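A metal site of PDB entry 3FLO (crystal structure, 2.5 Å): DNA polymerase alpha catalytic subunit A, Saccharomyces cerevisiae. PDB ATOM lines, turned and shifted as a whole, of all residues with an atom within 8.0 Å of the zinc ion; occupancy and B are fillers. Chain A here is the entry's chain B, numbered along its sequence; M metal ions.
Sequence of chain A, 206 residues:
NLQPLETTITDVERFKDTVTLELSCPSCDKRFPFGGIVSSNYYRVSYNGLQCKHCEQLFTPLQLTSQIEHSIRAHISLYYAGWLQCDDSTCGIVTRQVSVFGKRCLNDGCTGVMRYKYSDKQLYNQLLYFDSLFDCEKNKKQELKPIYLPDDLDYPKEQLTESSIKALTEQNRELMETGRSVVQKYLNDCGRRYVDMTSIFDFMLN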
ATOM      1  N   SER A  24      20.549   7.881 -31.063  1.00  0.00           N
ATOM      2  CA  SER A  24      21.393   7.103 -30.242  1.00  0.00           C
ATOM      3  C   SER A  24      22.739   7.821 -30.133  1.00  0.00           C
ATOM      4  O   SER A  24      23.215   8.402 -31.099  1.00  0.00           O
ATOM      5  CB  SER A  24      21.554   5.730 -30.860  1.00  0.00           C
ATOM      6  OG  SER A  24      21.757   4.785 -29.817  1.00  0.00           O
ATOM      7  N   CYS A  25      23.323   7.807 -28.943  1.00  0.00           N
ATOM      8  CA  CYS A  25      24.570   8.533 -28.696  1.00  0.00           C
ATOM      9  C   CYS A  25      25.757   7.754 -29.222  1.00  0.00           C
ATOM     10  O   CYS A  25      25.913   6.605 -28.862  1.00  0.00           O
ATOM     11  CB  CYS A  25      24.768   8.839 -27.203  1.00  0.00           C
ATOM     12  SG  CYS A  25      26.441   9.482 -26.795  1.00  0.00           S
ATOM     13  N   PRO A  26      26.558   8.366 -30.090  1.00  0.00           N
ATOM     14  CA  PRO A  26      27.680   7.624 -30.658  1.00  0.00           C
ATOM     15  C   PRO A  26      28.682   7.069 -29.650  1.00  0.00           C
ATOM     16  O   PRO A  26      29.230   5.998 -29.923  1.00  0.00           O
ATOM     17  CB  PRO A  26      28.344   8.648 -31.589  1.00  0.00           C
ATOM     18  CG  PRO A  26      27.257   9.671 -31.833  1.00  0.00           C
ATOM     19  CD  PRO A  26      26.445   9.721 -30.644  1.00  0.00           C
ATOM     20  N   SER A  27      28.940   7.776 -28.534  1.00  0.00           N
ATOM     21  CA  SER A  27      29.938   7.314 -27.561  1.00  0.00           C
ATOM     22  C   SER A  27      29.360   6.222 -26.667  1.00  0.00           C
ATOM     23  O   SER A  27      29.965   5.163 -26.513  1.00  0.00           O
ATOM     24  CB  SER A  27      30.504   8.423 -26.628  1.00  0.00           C
ATOM     25  OG  SER A  27      30.701   9.680 -27.288  1.00  0.00           O
ATOM     26  N   CYS A  28      28.224   6.504 -26.030  1.00  0.00           N
ATOM     27  CA  CYS A  28      27.779   5.658 -24.934  1.00  0.00           C
ATOM     28  C   CYS A  28      26.533   4.836 -25.245  1.00  0.00           C
ATOM     29  O   CYS A  28      26.197   3.949 -24.478  1.00  0.00           O
ATOM     30  CB  CYS A  28      27.538   6.515 -23.693  1.00  0.00           C
ATOM     31  SG  CYS A  28      26.024   7.454 -23.737  1.00  0.00           S
ATOM     32  N   ASP A  29      25.873   5.111 -26.364  1.00  0.00           N
ATOM     33  CA  ASP A  29      24.783   4.285 -26.906  1.00  0.00           C
ATOM     34  C   ASP A  29      23.427   4.510 -26.246  1.00  0.00           C
ATOM     35  O   ASP A  29      22.472   3.851 -26.602  1.00  0.00           O
ATOM     36  CB  ASP A  29      25.089   2.781 -26.891  1.00  0.00           C
ATOM     37  CG  ASP A  29      26.269   2.396 -27.767  1.00  0.00           C
ATOM     38  OD1 ASP A  29      26.644   3.148 -28.712  1.00  0.00           O
ATOM     39  OD2 ASP A  29      26.829   1.323 -27.495  1.00  0.00           O
ATOM     40  N   LYS A  30      23.327   5.472 -25.335  1.00  0.00           N
ATOM     41  CA  LYS A  30      22.033   5.788 -24.755  1.00  0.00           C
ATOM     42  C   LYS A  30      21.101   6.317 -25.854  1.00  0.00           C
ATOM     43  O   LYS A  30      21.517   7.088 -26.736  1.00  0.00           O
ATOM     44  CB  LYS A  30      22.196   6.815 -23.605  1.00  0.00           C
ATOM     45  CG  LYS A  30      21.360   6.534 -22.298  1.00  0.00           C
ATOM     46  CD  LYS A  30      22.132   5.598 -21.372  1.00  0.00           C
ATOM     47  CE  LYS A  30      21.372   5.317 -20.044  1.00  0.00           C
ATOM     48  NZ  LYS A  30      20.447   6.450 -19.587  1.00  0.00           N
ATOM     49  N   ARG A  31      19.846   5.835 -25.838  1.00  0.00           N
ATOM     50  CA  ARG A  31      18.849   6.196 -26.839  1.00  0.00           C
ATOM     51  C   ARG A  31      17.882   7.192 -26.270  1.00  0.00           C
ATOM     52  O   ARG A  31      17.518   7.059 -25.123  1.00  0.00           O
ATOM     53  CB  ARG A  31      18.064   4.954 -27.300  1.00  0.00           C
ATOM     54  CG  ARG A  31      18.950   3.897 -27.915  1.00  0.00           C
ATOM     55  CD  ARG A  31      18.190   2.795 -28.715  1.00  0.00           C
ATOM     56  NE  ARG A  31      16.759   3.128 -28.918  1.00  0.00           N
ATOM     57  CZ  ARG A  31      16.176   3.531 -30.059  1.00  0.00           C
ATOM     58  NH1 ARG A  31      16.873   3.706 -31.196  1.00  0.00           N
ATOM     59  NH2 ARG A  31      14.854   3.785 -30.069  1.00  0.00           N
ATOM     60  N   PHE A  32      17.465   8.174 -27.056  1.00  0.00           N
ATOM     61  CA  PHE A  32      16.534   9.182 -26.579  1.00  0.00           C
ATOM     62  C   PHE A  32      15.783   9.881 -27.695  1.00  0.00           C
ATOM     63  O   PHE A  32      16.295   9.962 -28.807  1.00  0.00           O
ATOM     64  CB  PHE A  32      17.280  10.211 -25.716  1.00  0.00           C
ATOM     65  CG  PHE A  32      18.375  10.928 -26.428  1.00  0.00           C
ATOM     66  CD1 PHE A  32      19.699  10.553 -26.264  1.00  0.00           C
ATOM     67  CD2 PHE A  32      18.107  12.028 -27.233  1.00  0.00           C
ATOM     68  CE1 PHE A  32      20.708  11.219 -26.924  1.00  0.00           C
ATOM     69  CE2 PHE A  32      19.117  12.711 -27.890  1.00  0.00           C
ATOM     70  CZ  PHE A  32      20.402  12.317 -27.744  1.00  0.00           C
ATOM     71  N   TYR A  42      17.942  14.010 -21.243  1.00  0.00           N
ATOM     72  CA  TYR A  42      18.918  13.172 -21.987  1.00  0.00           C
ATOM     73  C   TYR A  42      19.903  13.932 -22.804  1.00  0.00           C
ATOM     74  O   TYR A  42      20.973  13.442 -23.072  1.00  0.00           O
ATOM     75  CB  TYR A  42      18.240  12.172 -22.957  1.00  0.00           C
ATOM     76  CG  TYR A  42      17.451  11.189 -22.184  1.00  0.00           C
ATOM     77  CD1 TYR A  42      18.056  10.056 -21.673  1.00  0.00           C
ATOM     78  CD2 TYR A  42      16.129  11.446 -21.888  1.00  0.00           C
ATOM     79  CE1 TYR A  42      17.334   9.163 -20.901  1.00  0.00           C
ATOM     80  CE2 TYR A  42      15.409  10.575 -21.106  1.00  0.00           C
ATOM     81  CZ  TYR A  42      16.023   9.428 -20.623  1.00  0.00           C
ATOM     82  OH  TYR A  42      15.288   8.570 -19.845  1.00  0.00           O
ATOM     83  N   GLN A  51      24.464  17.817 -27.361  1.00  0.00           N
ATOM     84  CA  GLN A  51      25.271  17.123 -26.383  1.00  0.00           C
ATOM     85  C   GLN A  51      24.494  16.117 -25.578  1.00  0.00           C
ATOM     86  O   GLN A  51      23.415  16.404 -25.033  1.00  0.00           O
ATOM     87  CB  GLN A  51      25.925  18.108 -25.424  1.00  0.00           C
ATOM     88  CG  GLN A  51      26.904  17.467 -24.458  1.00  0.00           C
ATOM     89  CD  GLN A  51      27.686  18.536 -23.599  1.00  0.00           C
ATOM     90  OE1 GLN A  51      27.396  19.723 -23.647  1.00  0.00           O
ATOM     91  NE2 GLN A  51      28.644  18.074 -22.824  1.00  0.00           N
ATOM     92  N   CYS A  52      25.091  14.946 -25.455  1.00  0.00           N
ATOM     93  CA  CYS A  52      24.562  13.878 -24.662  1.00  0.00           C
ATOM     94  C   CYS A  52      24.749  14.109 -23.174  1.00  0.00           C
ATOM     95  O   CYS A  52      25.882  14.304 -22.724  1.00  0.00           O
ATOM     96  CB  CYS A  52      25.286  12.599 -25.053  1.00  0.00           C
ATOM     97  SG  CYS A  52      24.933  11.232 -23.978  1.00  0.00           S
ATOM     98  N   LYS A  53      23.674  14.071 -22.394  1.00  0.00           N
ATOM     99  CA  LYS A  53      23.813  14.374 -20.947  1.00  0.00           C
ATOM    100  C   LYS A  53      24.405  13.229 -20.130  1.00  0.00           C
ATOM    101  O   LYS A  53      24.977  13.465 -19.089  1.00  0.00           O
ATOM    102  CB  LYS A  53      22.503  14.846 -20.308  1.00  0.00           C
ATOM    103  CG  LYS A  53      22.150  16.274 -20.595  1.00  0.00           C
ATOM    104  CD  LYS A  53      20.852  16.680 -19.913  1.00  0.00           C
ATOM    105  CE  LYS A  53      20.485  18.155 -20.199  1.00  0.00           C
ATOM    106  NZ  LYS A  53      19.330  18.661 -19.321  1.00  0.00           N
ATOM    107  N   HIS A  54      24.278  11.993 -20.598  1.00  0.00           N
ATOM    108  CA  HIS A  54      24.795  10.853 -19.840  1.00  0.00           C
ATOM    109  C   HIS A  54      26.327  10.815 -19.852  1.00  0.00           C
ATOM    110  O   HIS A  54      26.936  10.532 -18.823  1.00  0.00           O
ATOM    111  CB  HIS A  54      24.271   9.533 -20.364  1.00  0.00           C
ATOM    112  CG  HIS A  54      24.792   8.347 -19.617  1.00  0.00           C
ATOM    113  ND1 HIS A  54      25.764   7.512 -20.133  1.00  0.00           N
ATOM    114  CD2 HIS A  54      24.517   7.898 -18.368  1.00  0.00           C
ATOM    115  CE1 HIS A  54      26.057   6.579 -19.237  1.00  0.00           C
ATOM    116  NE2 HIS A  54      25.324   6.793 -18.157  1.00  0.00           N
ATOM    117  N   CYS A  55      26.944  11.096 -21.007  1.00  0.00           N
ATOM    118  CA  CYS A  55      28.406  11.036 -21.133  1.00  0.00           C
ATOM    119  C   CYS A  55      29.086  12.356 -21.570  1.00  0.00           C
ATOM    120  O   CYS A  55      30.305  12.402 -21.708  1.00  0.00           O
ATOM    121  CB  CYS A  55      28.781   9.923 -22.094  1.00  0.00           C
ATOM    122  SG  CYS A  55      28.657  10.362 -23.848  1.00  0.00           S
ATOM    123  N   GLU A  56      28.297  13.399 -21.797  1.00  0.00           N
ATOM    124  CA  GLU A  56      28.830  14.711 -22.170  1.00  0.00           C
ATOM    125  C   GLU A  56      29.445  14.834 -23.573  1.00  0.00           C
ATOM    126  O   GLU A  56      29.909  15.898 -23.943  1.00  0.00           O
ATOM    127  CB  GLU A  56      29.862  15.198 -21.112  1.00  0.00           C
ATOM    128  CG  GLU A  56      29.301  15.229 -19.662  1.00  0.00           C
ATOM    129  CD  GLU A  56      28.165  16.241 -19.515  1.00  0.00           C
ATOM    130  OE1 GLU A  56      28.316  17.336 -20.130  1.00  0.00           O
ATOM    131  OE2 GLU A  56      27.107  15.955 -18.850  1.00  0.00           O
ATOM    132  N   GLN A  57      29.411  13.770 -24.373  1.00  0.00           N
ATOM    133  CA  GLN A  57      29.981  13.849 -25.700  1.00  0.00           C
ATOM    134  C   GLN A  57      29.073  14.566 -26.683  1.00  0.00           C
ATOM    135  O   GLN A  57      27.846  14.438 -26.628  1.00  0.00           O
ATOM    136  CB  GLN A  57      30.371  12.470 -26.232  1.00  0.00           C
ATOM    137  CG  GLN A  57      31.757  11.885 -25.629  1.00  0.00           C
ATOM    138  CD  GLN A  57      32.924  12.890 -25.637  1.00  0.00           C
ATOM    139  OE1 GLN A  57      33.212  13.500 -26.663  1.00  0.00           O
ATOM    140  NE2 GLN A  57      33.607  13.053 -24.486  1.00  0.00           N
ATOM    141  N   LEU A  58      29.699  15.348 -27.551  1.00  0.00           N
ATOM    142  CA  LEU A  58      29.027  16.161 -28.547  1.00  0.00           C
ATOM    143  C   LEU A  58      28.788  15.356 -29.797  1.00  0.00           C
ATOM    144  O   LEU A  58      29.696  14.718 -30.245  1.00  0.00           O
ATOM    145  CB  LEU A  58      29.939  17.279 -28.989  1.00  0.00           C
ATOM    146  CG  LEU A  58      29.922  18.584 -28.224  1.00  0.00           C
ATOM    147  CD1 LEU A  58      31.194  19.400 -28.620  1.00  0.00           C
ATOM    148  CD2 LEU A  58      28.590  19.324 -28.529  1.00  0.00           C
ATOM    149  N   PHE A  59      27.590  15.437 -30.368  1.00  0.00           N
ATOM    150  CA  PHE A  59      27.359  14.839 -31.681  1.00  0.00           C
ATOM    151  C   PHE A  59      28.066  15.694 -32.715  1.00  0.00           C
ATOM    152  O   PHE A  59      28.006  16.905 -32.634  1.00  0.00           O
ATOM    153  CB  PHE A  59      25.891  14.872 -32.064  1.00  0.00           C
ATOM    154  CG  PHE A  59      25.069  13.834 -31.394  1.00  0.00           C
ATOM    155  CD1 PHE A  59      24.960  13.785 -30.016  1.00  0.00           C
ATOM    156  CD2 PHE A  59      24.326  12.931 -32.163  1.00  0.00           C
ATOM    157  CE1 PHE A  59      24.183  12.845 -29.394  1.00  0.00           C
ATOM    158  CE2 PHE A  59      23.523  11.985 -31.567  1.00  0.00           C
ATOM    159  CZ  PHE A  59      23.453  11.925 -30.168  1.00  0.00           C
HETATM  160 ZN    ZN M   1      26.507   9.584 -24.433  1.00  0.00          ZN
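The backbone NH (N) of His 54 sits close to the side-chain sulfur (SG) of Cys 52 (3.5 Å).
The backbone NH (N) of Ser 27 lies close to the side-chain sulfur (SG) of Cys 25 (3.5 Å).
O of Gln 57 lies within hydrogen-bond range of N of Cys 52 (3.0 Å).
The side-chain sulfur (SG) of Cys 28 sits close to the backbone NH (N) of Lys 30, 3.7 Å away.
N of Gln 57 sits close to SG of Cys 55, at 3.5 Å.
The backbone NH of Cys 25 is in hydrogen-bond range of the backbone carbonyl oxygen of Lys 30, 2.9 Å away.
The side-chain sulfur (SG) of Cys 28 sits close to a ring nitrogen (ND1) of His 54 (3.6 Å).
The zinc ion is bound by the side-chain sulfur of Cys 28 (2.3 Å), the side-chain sulfur of Cys 52 (2.3 Å), the side-chain sulfur of Cys 55 (2.4 Å) and the side-chain sulfur of Cys 25 (2.4 Å).
The zinc ion has four donor atoms within binding distance.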
